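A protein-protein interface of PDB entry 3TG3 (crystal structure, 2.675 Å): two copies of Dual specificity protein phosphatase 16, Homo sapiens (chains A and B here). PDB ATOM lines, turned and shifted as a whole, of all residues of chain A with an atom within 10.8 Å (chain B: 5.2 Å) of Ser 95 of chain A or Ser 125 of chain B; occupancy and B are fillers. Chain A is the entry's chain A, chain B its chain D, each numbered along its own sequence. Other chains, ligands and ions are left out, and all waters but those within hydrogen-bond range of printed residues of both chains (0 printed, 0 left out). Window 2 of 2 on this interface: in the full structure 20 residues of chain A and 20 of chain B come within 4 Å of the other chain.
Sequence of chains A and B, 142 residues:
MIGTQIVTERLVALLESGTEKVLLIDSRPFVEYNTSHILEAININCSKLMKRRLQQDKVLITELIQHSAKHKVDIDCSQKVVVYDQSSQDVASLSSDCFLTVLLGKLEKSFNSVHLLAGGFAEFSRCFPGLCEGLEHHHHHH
OG of Ser 95 of chain A sits close to NE2 of Gln 86 of chain B.
The side-chain carboxylate (OD1) of Asp 90 of chain A sits close to the backbone NH (N) of Ala 92 of chain A, at 3.4 Å. The backbone carbonyl oxygen (O) of Asp 90 of chain A lies within hydrogen-bond range of the side-chain hydroxyl (OG) of Ser 93 of chain A, at 3.1 Å. O of Ser 95 of chain A sits at hydrogen-bond distance from SG of Cys 98 of chain A. The side-chain hydroxyl (OG1) of Thr 101 of chain A sits at hydrogen-bond distance from the backbone carbonyl oxygen (O) of Ser 95 of chain A (3.3 Å). The backbone NH of Ala 122 of chain B is in hydrogen-bond range of the backbone carbonyl oxygen of Gln 86 of chain B, 2.7 Å away. O of Ala 122 of chain B is in hydrogen-bond range of OG of Ser 125 of chain B (3.3 Å).
Among the printed residues, merely in contact across the chains: Ser 93 of chain A with Arg 126 of chain B, Ser 93 of chain A with Ala 122 of chain B, Ser 95 of chain A with Ser 125 of chain B, Cys 98 of chain A with Gln 86 of chain B and Ala 92 of chain A with Arg 126 of chain B.
Of the printed residues of chain B, Ser 93 of chain A touches Ala 122 (3.6 Å) and Arg 126 (3.4 Å). Of the printed residues of chain B, Ser 95 of chain A touches Gln 86 and Ser 125. Of the printed residues of chain B, Cys 98 of chain A touches Gln 86 (3.7 Å). Leu 103 of chain A touches none of the printed residues of chain B. Gly 105 of chain A touches none of the printed residues of chain B. No residue of chain A comes within 4 Å of Phe 121 of chain B. Printed residues of chain A within 4 Å of Ala 122 of chain B: Ser 93 (3.6 Å). No residue of chain A comes within 4 Å of Phe 124 of chain B. Ser 125 of chain B touches just one residue of chain A: Ser 95. No residue of chain A comes within 4 Å of Cys 127 of chain B. No residue of chain A comes within 4 Å of Pro 129 of chain B. The nearest printed residue of chain B that does not touch Ser 95 of chain A is Ala 122 of chain B (4.0004 Å).
Hydrophobic or aromatic side chains of chain B that line the printed part of chain A: Ala 122.
No position is printed for both chains.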
ATOM      1  N   CYS A  46      25.280   4.013  24.909  1.00  0.00           N
ATOM      2  CA  CYS A  46      24.067   4.801  24.796  1.00  0.00           C
ATOM      3  C   CYS A  46      24.461   6.254  24.669  1.00  0.00           C
ATOM      4  O   CYS A  46      24.889   6.893  25.628  1.00  0.00           O
ATOM      5  CB  CYS A  46      23.182   4.583  26.017  1.00  0.00           C
ATOM      6  SG  CYS A  46      21.773   5.704  26.137  1.00  0.00           S
ATOM      7  N   LYS A  51      22.950   6.636  18.920  1.00  0.00           N
ATOM      8  CA  LYS A  51      21.545   6.330  18.728  1.00  0.00           C
ATOM      9  C   LYS A  51      21.065   6.868  17.401  1.00  0.00           C
ATOM     10  O   LYS A  51      20.333   6.195  16.684  1.00  0.00           O
ATOM     11  CB  LYS A  51      20.706   6.894  19.880  1.00  0.00           C
ATOM     12  CG  LYS A  51      19.234   6.504  19.819  1.00  0.00           C
ATOM     13  CD  LYS A  51      18.480   7.015  21.018  1.00  0.00           C
ATOM     14  CE  LYS A  51      16.995   6.644  20.939  1.00  0.00           C
ATOM     15  NZ  LYS A  51      16.270   6.930  22.222  1.00  0.00           N
ATOM     16  N   GLN A  55      19.688   4.142  14.366  1.00  0.00           N
ATOM     17  CA  GLN A  55      18.340   4.229  13.822  1.00  0.00           C
ATOM     18  C   GLN A  55      18.276   4.980  12.485  1.00  0.00           C
ATOM     19  O   GLN A  55      17.309   4.844  11.733  1.00  0.00           O
ATOM     20  CB  GLN A  55      17.364   4.813  14.852  1.00  0.00           C
ATOM     21  CG  GLN A  55      17.651   6.227  15.284  1.00  0.00           C
ATOM     22  CD  GLN A  55      16.638   6.727  16.291  1.00  0.00           C
ATOM     23  OE1 GLN A  55      16.671   7.891  16.704  1.00  0.00           O
ATOM     24  NE2 GLN A  55      15.724   5.850  16.692  1.00  0.00           N
ATOM     25  N   ASP A  85      22.175  -3.808  29.680  1.00  0.00           N
ATOM     26  CA  ASP A  85      22.262  -2.472  30.242  1.00  0.00           C
ATOM     27  C   ASP A  85      22.523  -2.668  31.712  1.00  0.00           C
ATOM     28  O   ASP A  85      23.041  -3.705  32.128  1.00  0.00           O
ATOM     29  CB  ASP A  85      20.971  -1.689  30.045  1.00  0.00           C
ATOM     30  CG  ASP A  85      19.759  -2.430  30.557  1.00  0.00           C
ATOM     31  OD1 ASP A  85      19.895  -3.249  31.496  1.00  0.00           O
ATOM     32  OD2 ASP A  85      18.661  -2.187  30.024  1.00  0.00           O
ATOM     33  N   SER A  88      17.908  -3.968  33.126  1.00  0.00           N
ATOM     34  CA  SER A  88      16.728  -4.489  32.452  1.00  0.00           C
ATOM     35  C   SER A  88      16.588  -5.990  32.648  1.00  0.00           C
ATOM     36  O   SER A  88      17.555  -6.728  32.483  1.00  0.00           O
ATOM     37  CB  SER A  88      16.751  -4.154  30.965  1.00  0.00           C
ATOM     38  OG  SER A  88      16.308  -2.821  30.741  1.00  0.00           O
ATOM     39  N   GLN A  89      15.383  -6.434  32.996  1.00  0.00           N
ATOM     40  CA  GLN A  89      15.124  -7.857  33.217  1.00  0.00           C
ATOM     41  C   GLN A  89      14.869  -8.619  31.921  1.00  0.00           C
ATOM     42  O   GLN A  89      15.440  -9.684  31.711  1.00  0.00           O
ATOM     43  CB  GLN A  89      13.962  -8.070  34.197  1.00  0.00           C
ATOM     44  CG  GLN A  89      14.348  -7.949  35.667  1.00  0.00           C
ATOM     45  CD  GLN A  89      15.178  -9.128  36.160  1.00  0.00           C
ATOM     46  OE1 GLN A  89      14.908 -10.287  35.831  1.00  0.00           O
ATOM     47  NE2 GLN A  89      16.192  -8.833  36.964  1.00  0.00           N
ATOM     48  N   ASP A  90      14.005  -8.084  31.064  1.00  0.00           N
ATOM     49  CA  ASP A  90      13.686  -8.759  29.807  1.00  0.00           C
ATOM     50  C   ASP A  90      13.224  -7.814  28.695  1.00  0.00           C
ATOM     51  O   ASP A  90      13.046  -6.619  28.921  1.00  0.00           O
ATOM     52  CB  ASP A  90      12.664  -9.887  30.027  1.00  0.00           C
ATOM     53  CG  ASP A  90      11.361  -9.404  30.667  1.00  0.00           C
ATOM     54  OD1 ASP A  90      10.802  -8.378  30.216  1.00  0.00           O
ATOM     55  OD2 ASP A  90      10.889 -10.073  31.616  1.00  0.00           O
ATOM     56  N   VAL A  91      13.028  -8.362  27.500  1.00  0.00           N
ATOM     57  CA  VAL A  91      12.725  -7.556  26.321  1.00  0.00           C
ATOM     58  C   VAL A  91      11.381  -6.825  26.406  1.00  0.00           C
ATOM     59  O   VAL A  91      11.270  -5.671  25.977  1.00  0.00           O
ATOM     60  CB  VAL A  91      12.761  -8.401  25.033  1.00  0.00           C
ATOM     61  CG1 VAL A  91      12.395  -7.546  23.818  1.00  0.00           C
ATOM     62  CG2 VAL A  91      14.133  -9.043  24.855  1.00  0.00           C
ATOM     63  N   ALA A  92      10.363  -7.494  26.950  1.00  0.00           N
ATOM     64  CA  ALA A  92       9.040  -6.890  27.085  1.00  0.00           C
ATOM     65  C   ALA A  92       9.078  -5.640  27.951  1.00  0.00           C
ATOM     66  O   ALA A  92       8.342  -4.688  27.700  1.00  0.00           O
ATOM     67  CB  ALA A  92       8.067  -7.892  27.656  1.00  0.00           C
ATOM     68  N   SER A  93       9.933  -5.648  28.972  1.00  0.00           N
ATOM     69  CA  SER A  93      10.069  -4.499  29.863  1.00  0.00           C
ATOM     70  C   SER A  93      11.081  -3.472  29.339  1.00  0.00           C
ATOM     71  O   SER A  93      11.869  -2.921  30.109  1.00  0.00           O
ATOM     72  CB  SER A  93      10.427  -4.945  31.291  1.00  0.00           C
ATOM     73  OG  SER A  93      11.773  -5.377  31.402  1.00  0.00           O
ATOM     74  N   LEU A  94      11.058  -3.221  28.031  1.00  0.00           N
ATOM     75  CA  LEU A  94      11.860  -2.144  27.442  1.00  0.00           C
ATOM     76  C   LEU A  94      10.943  -1.069  26.887  1.00  0.00           C
ATOM     77  O   LEU A  94       9.988  -1.388  26.177  1.00  0.00           O
ATOM     78  CB  LEU A  94      12.747  -2.658  26.304  1.00  0.00           C
ATOM     79  CG  LEU A  94      13.882  -3.646  26.583  1.00  0.00           C
ATOM     80  CD1 LEU A  94      14.713  -3.843  25.322  1.00  0.00           C
ATOM     81  CD2 LEU A  94      14.763  -3.185  27.743  1.00  0.00           C
ATOM     82  N   SER A  95      11.221   0.193  27.207  1.00  0.00           N
ATOM     83  CA  SER A  95      10.379   1.277  26.720  1.00  0.00           C
ATOM     84  C   SER A  95      10.519   1.286  25.210  1.00  0.00           C
ATOM     85  O   SER A  95      11.622   1.170  24.681  1.00  0.00           O
ATOM     86  CB  SER A  95      10.774   2.622  27.324  1.00  0.00           C
ATOM     87  OG  SER A  95      11.594   3.359  26.447  1.00  0.00           O
ATOM     88  N   SER A  96       9.396   1.394  24.516  1.00  0.00           N
ATOM     89  CA  SER A  96       9.370   1.094  23.093  1.00  0.00           C
ATOM     90  C   SER A  96      10.476   1.757  22.263  1.00  0.00           C
ATOM     91  O   SER A  96      10.900   1.201  21.260  1.00  0.00           O
ATOM     92  CB  SER A  96       7.991   1.406  22.499  1.00  0.00           C
ATOM     93  OG  SER A  96       7.889   2.774  22.158  1.00  0.00           O
ATOM     94  N   ASP A  97      10.938   2.939  22.659  1.00  0.00           N
ATOM     95  CA  ASP A  97      11.914   3.655  21.845  1.00  0.00           C
ATOM     96  C   ASP A  97      13.175   4.068  22.629  1.00  0.00           C
ATOM     97  O   ASP A  97      13.737   5.149  22.416  1.00  0.00           O
ATOM     98  CB  ASP A  97      11.266   4.872  21.180  1.00  0.00           C
ATOM     99  CG  ASP A  97      12.231   5.624  20.258  1.00  0.00           C
ATOM    100  OD1 ASP A  97      11.933   6.779  19.883  1.00  0.00           O
ATOM    101  OD2 ASP A  97      13.296   5.065  19.911  1.00  0.00           O
ATOM    102  N   CYS A  98      13.619   3.200  23.532  1.00  0.00           N
ATOM    103  CA  CYS A  98      14.845   3.444  24.285  1.00  0.00           C
ATOM    104  C   CYS A  98      16.049   2.975  23.480  1.00  0.00           C
ATOM    105  O   CYS A  98      15.897   2.202  22.533  1.00  0.00           O
ATOM    106  CB  CYS A  98      14.791   2.715  25.618  1.00  0.00           C
ATOM    107  SG  CYS A  98      14.801   0.936  25.417  1.00  0.00           S
ATOM    108  N   PHE A  99      17.240   3.449  23.839  1.00  0.00           N
ATOM    109  CA  PHE A  99      18.459   3.067  23.096  1.00  0.00           C
ATOM    110  C   PHE A  99      18.642   1.551  22.902  1.00  0.00           C
ATOM    111  O   PHE A  99      18.767   1.070  21.786  1.00  0.00           O
ATOM    112  CB  PHE A  99      19.703   3.628  23.770  1.00  0.00           C
ATOM    113  CG  PHE A  99      20.963   3.267  23.070  1.00  0.00           C
ATOM    114  CD1 PHE A  99      21.386   3.993  21.963  1.00  0.00           C
ATOM    115  CD2 PHE A  99      21.723   2.192  23.492  1.00  0.00           C
ATOM    116  CE1 PHE A  99      22.556   3.664  21.294  1.00  0.00           C
ATOM    117  CE2 PHE A  99      22.896   1.851  22.825  1.00  0.00           C
ATOM    118  CZ  PHE A  99      23.309   2.595  21.726  1.00  0.00           C
ATOM    119  N   LEU A 100      18.659   0.813  24.009  1.00  0.00           N
ATOM    120  CA  LEU A 100      18.732  -0.642  23.995  1.00  0.00           C
ATOM    121  C   LEU A 100      17.886  -1.261  22.896  1.00  0.00           C
ATOM    122  O   LEU A 100      18.382  -2.028  22.071  1.00  0.00           O
ATOM    123  CB  LEU A 100      18.259  -1.186  25.344  1.00  0.00           C
ATOM    124  CG  LEU A 100      18.403  -2.689  25.560  1.00  0.00           C
ATOM    125  CD1 LEU A 100      19.749  -3.178  24.979  1.00  0.00           C
ATOM    126  CD2 LEU A 100      18.316  -3.001  27.029  1.00  0.00           C
ATOM    127  N   THR A 101      16.601  -0.940  22.934  1.00  0.00           N
ATOM    128  CA  THR A 101      15.617  -1.343  21.939  1.00  0.00           C
ATOM    129  C   THR A 101      16.095  -1.061  20.509  1.00  0.00           C
ATOM    130  O   THR A 101      16.137  -1.974  19.663  1.00  0.00           O
ATOM    131  CB  THR A 101      14.296  -0.586  22.213  1.00  0.00           C
ATOM    132  OG1 THR A 101      13.687  -1.098  23.401  1.00  0.00           O
ATOM    133  CG2 THR A 101      13.335  -0.728  21.098  1.00  0.00           C
ATOM    134  N   VAL A 102      16.447   0.197  20.236  1.00  0.00           N
ATOM    135  CA  VAL A 102      16.993   0.570  18.931  1.00  0.00           C
ATOM    136  C   VAL A 102      18.072  -0.440  18.531  1.00  0.00           C
ATOM    137  O   VAL A 102      18.010  -1.061  17.457  1.00  0.00           O
ATOM    138  CB  VAL A 102      17.616   1.977  18.967  1.00  0.00           C
ATOM    139  CG1 VAL A 102      18.455   2.223  17.716  1.00  0.00           C
ATOM    140  CG2 VAL A 102      16.547   3.031  19.135  1.00  0.00           C
ATOM    141  N   LEU A 103      19.049  -0.590  19.428  1.00  0.00           N
ATOM    142  CA  LEU A 103      20.179  -1.478  19.241  1.00  0.00           C
ATOM    143  C   LEU A 103      19.711  -2.906  18.978  1.00  0.00           C
ATOM    144  O   LEU A 103      20.123  -3.540  18.005  1.00  0.00           O
ATOM    145  CB  LEU A 103      21.067  -1.447  20.482  1.00  0.00           C
ATOM    146  CG  LEU A 103      22.315  -2.310  20.410  1.00  0.00           C
ATOM    147  CD1 LEU A 103      23.343  -1.623  19.525  1.00  0.00           C
ATOM    148  CD2 LEU A 103      22.885  -2.559  21.795  1.00  0.00           C
ATOM    149  N   LEU A 104      18.847  -3.412  19.848  1.00  0.00           N
ATOM    150  CA  LEU A 104      18.381  -4.786  19.710  1.00  0.00           C
ATOM    151  C   LEU A 104      17.864  -5.081  18.305  1.00  0.00           C
ATOM    152  O   LEU A 104      18.007  -6.185  17.805  1.00  0.00           O
ATOM    153  CB  LEU A 104      17.304  -5.112  20.751  1.00  0.00           C
ATOM    154  CG  LEU A 104      17.785  -5.413  22.178  1.00  0.00           C
ATOM    155  CD1 LEU A 104      16.611  -5.723  23.093  1.00  0.00           C
ATOM    156  CD2 LEU A 104      18.781  -6.559  22.220  1.00  0.00           C
ATOM    157  N   GLY A 105      17.265  -4.090  17.669  1.00  0.00           N
ATOM    158  CA  GLY A 105      16.768  -4.283  16.321  1.00  0.00           C
ATOM    159  C   GLY A 105      17.884  -4.550  15.337  1.00  0.00           C
ATOM    160  O   GLY A 105      17.897  -5.585  14.672  1.00  0.00           O
ATOM    161  N   LEU A 116      19.326 -11.003  25.605  1.00  0.00           N
ATOM    162  CA  LEU A 116      19.513  -9.957  26.582  1.00  0.00           C
ATOM    163  C   LEU A 116      19.935 -10.579  27.914  1.00  0.00           C
ATOM    164  O   LEU A 116      19.395 -11.612  28.326  1.00  0.00           O
ATOM    165  CB  LEU A 116      18.197  -9.192  26.749  1.00  0.00           C
ATOM    166  CG  LEU A 116      18.124  -8.104  27.819  1.00  0.00           C
ATOM    167  CD1 LEU A 116      18.939  -6.872  27.383  1.00  0.00           C
ATOM    168  CD2 LEU A 116      16.657  -7.741  28.128  1.00  0.00           C
ATOM    169  N   GLN B  86      16.325   3.880  33.759  1.00  0.00           N
ATOM    170  CA  GLN B  86      15.486   3.230  32.768  1.00  0.00           C
ATOM    171  C   GLN B  86      14.701   2.062  33.331  1.00  0.00           C
ATOM    172  O   GLN B  86      13.549   1.864  32.950  1.00  0.00           O
ATOM    173  CB  GLN B  86      16.313   2.790  31.570  1.00  0.00           C
ATOM    174  CG  GLN B  86      15.505   2.190  30.434  1.00  0.00           C
ATOM    175  CD  GLN B  86      14.692   3.220  29.679  1.00  0.00           C
ATOM    176  OE1 GLN B  86      15.073   4.390  29.573  1.00  0.00           O
ATOM    177  NE2 GLN B  86      13.560   2.782  29.145  1.00  0.00           N
ATOM    178  N   PHE B 121      12.002   4.260  34.194  1.00  0.00           N
ATOM    179  CA  PHE B 121      11.187   4.895  33.173  1.00  0.00           C
ATOM    180  C   PHE B 121      10.527   3.908  32.239  1.00  0.00           C
ATOM    181  O   PHE B 121       9.530   4.224  31.602  1.00  0.00           O
ATOM    182  CB  PHE B 121      12.015   5.870  32.356  1.00  0.00           C
ATOM    183  CG  PHE B 121      11.218   6.619  31.331  1.00  0.00           C
ATOM    184  CD1 PHE B 121      10.420   7.705  31.700  1.00  0.00           C
ATOM    185  CD2 PHE B 121      11.246   6.244  30.010  1.00  0.00           C
ATOM    186  CE1 PHE B 121       9.678   8.391  30.753  1.00  0.00           C
ATOM    187  CE2 PHE B 121      10.494   6.925  29.065  1.00  0.00           C
ATOM    188  CZ  PHE B 121       9.715   7.992  29.439  1.00  0.00           C
ATOM    189  N   ALA B 122      11.067   2.709  32.138  1.00  0.00           N
ATOM    190  CA  ALA B 122      10.437   1.734  31.259  1.00  0.00           C
ATOM    191  C   ALA B 122       9.023   1.457  31.742  1.00  0.00           C
ATOM    192  O   ALA B 122       8.103   1.355  30.929  1.00  0.00           O
ATOM    193  CB  ALA B 122      11.239   0.452  31.199  1.00  0.00           C
ATOM    194  N   GLU B 123       8.857   1.360  33.062  1.00  0.00           N
ATOM    195  CA  GLU B 123       7.587   0.920  33.636  1.00  0.00           C
ATOM    196  C   GLU B 123       6.578   2.036  33.742  1.00  0.00           C
ATOM    197  O   GLU B 123       5.381   1.822  33.560  1.00  0.00           O
ATOM    198  CB  GLU B 123       7.782   0.289  35.007  1.00  0.00           C
ATOM    199  CG  GLU B 123       6.485  -0.079  35.674  1.00  0.00           C
ATOM    200  CD  GLU B 123       6.648  -1.217  36.676  1.00  0.00           C
ATOM    201  OE1 GLU B 123       6.922  -2.356  36.233  1.00  0.00           O
ATOM    202  OE2 GLU B 123       6.493  -0.980  37.901  1.00  0.00           O
ATOM    203  N   PHE B 124       7.062   3.232  34.055  1.00  0.00           N
ATOM    204  CA  PHE B 124       6.185   4.374  34.121  1.00  0.00           C
ATOM    205  C   PHE B 124       5.648   4.688  32.747  1.00  0.00           C
ATOM    206  O   PHE B 124       4.465   4.956  32.594  1.00  0.00           O
ATOM    207  CB  PHE B 124       6.920   5.594  34.684  1.00  0.00           C
ATOM    208  CG  PHE B 124       6.042   6.813  34.835  1.00  0.00           C
ATOM    209  CD1 PHE B 124       5.640   7.246  36.093  1.00  0.00           C
ATOM    210  CD2 PHE B 124       5.623   7.521  33.726  1.00  0.00           C
ATOM    211  CE1 PHE B 124       4.855   8.366  36.234  1.00  0.00           C
ATOM    212  CE2 PHE B 124       4.822   8.636  33.858  1.00  0.00           C
ATOM    213  CZ  PHE B 124       4.439   9.058  35.108  1.00  0.00           C
ATOM    214  N   SER B 125       6.525   4.644  31.745  1.00  0.00           N
ATOM    215  CA  SER B 125       6.165   5.023  30.372  1.00  0.00           C
ATOM    216  C   SER B 125       5.244   3.982  29.753  1.00  0.00           C
ATOM    217  O   SER B 125       4.502   4.269  28.829  1.00  0.00           O
ATOM    218  CB  SER B 125       7.415   5.189  29.495  1.00  0.00           C
ATOM    219  OG  SER B 125       7.790   3.943  28.914  1.00  0.00           O
ATOM    220  N   ARG B 126       5.315   2.765  30.270  1.00  0.00           N
ATOM    221  CA  ARG B 126       4.457   1.686  29.816  1.00  0.00           C
ATOM    222  C   ARG B 126       3.056   1.951  30.333  1.00  0.00           C
ATOM    223  O   ARG B 126       2.081   1.826  29.603  1.00  0.00           O
ATOM    224  CB  ARG B 126       4.954   0.359  30.395  1.00  0.00           C
ATOM    225  CG  ARG B 126       4.389  -0.886  29.741  1.00  0.00           C
ATOM    226  CD  ARG B 126       5.450  -1.595  28.905  1.00  0.00           C
ATOM    227  NE  ARG B 126       6.713  -1.735  29.629  1.00  0.00           N
ATOM    228  CZ  ARG B 126       6.821  -2.188  30.876  1.00  0.00           C
ATOM    229  NH1 ARG B 126       5.731  -2.527  31.556  1.00  0.00           N
ATOM    230  NH2 ARG B 126       8.018  -2.289  31.451  1.00  0.00           N
ATOM    231  N   CYS B 127       2.975   2.330  31.606  1.00  0.00           N
ATOM    232  CA  CYS B 127       1.704   2.497  32.310  1.00  0.00           C
ATOM    233  C   CYS B 127       1.020   3.861  32.131  1.00  0.00           C
ATOM    234  O   CYS B 127      -0.205   3.938  32.213  1.00  0.00           O
ATOM    235  CB  CYS B 127       1.902   2.234  33.798  1.00  0.00           C
ATOM    236  SG  CYS B 127       2.439   0.566  34.181  1.00  0.00           S
ATOM    237  N   PHE B 128       1.801   4.921  31.878  1.00  0.00           N
ATOM    238  CA  PHE B 128       1.269   6.275  31.833  1.00  0.00           C
ATOM    239  C   PHE B 128       1.872   7.074  30.685  1.00  0.00           C
ATOM    240  O   PHE B 128       2.492   8.110  30.888  1.00  0.00           O
ATOM    241  CB  PHE B 128       1.486   6.990  33.189  1.00  0.00           C
ATOM    242  CG  PHE B 128       0.709   6.380  34.327  1.00  0.00           C
ATOM    243  CD1 PHE B 128       1.293   5.440  35.167  1.00  0.00           C
ATOM    244  CD2 PHE B 128      -0.614   6.729  34.546  1.00  0.00           C
ATOM    245  CE1 PHE B 128       0.578   4.857  36.196  1.00  0.00           C
ATOM    246  CE2 PHE B 128      -1.330   6.153  35.582  1.00  0.00           C
ATOM    247  CZ  PHE B 128      -0.722   5.208  36.406  1.00  0.00           C
ATOM    248  N   PRO B 129       1.668   6.601  29.461  1.00  0.00           N
ATOM    249  CA  PRO B 129       2.252   7.223  28.266  1.00  0.00           C
ATOM    250  C   PRO B 129       2.000   8.721  28.214  1.00  0.00           C
ATOM    251  O   PRO B 129       2.894   9.482  27.842  1.00  0.00           O
ATOM    252  CB  PRO B 129       1.499   6.543  27.132  1.00  0.00           C
ATOM    253  CG  PRO B 129       1.188   5.203  27.664  1.00  0.00           C
ATOM    254  CD  PRO B 129       0.856   5.420  29.121  1.00  0.00           C
ATOM    255  N   CYS B 132       4.202  11.511  29.888  1.00  0.00           N
ATOM    256  CA  CYS B 132       5.598  11.565  29.474  1.00  0.00           C
ATOM    257  C   CYS B 132       5.773  12.554  28.314  1.00  0.00           C
ATOM    258  O   CYS B 132       5.173  12.399  27.251  1.00  0.00           O
ATOM    259  CB  CYS B 132       6.110  10.169  29.089  1.00  0.00           C
ATOM    260  SG  CYS B 132       5.923   8.922  30.404  1.00  0.00           S
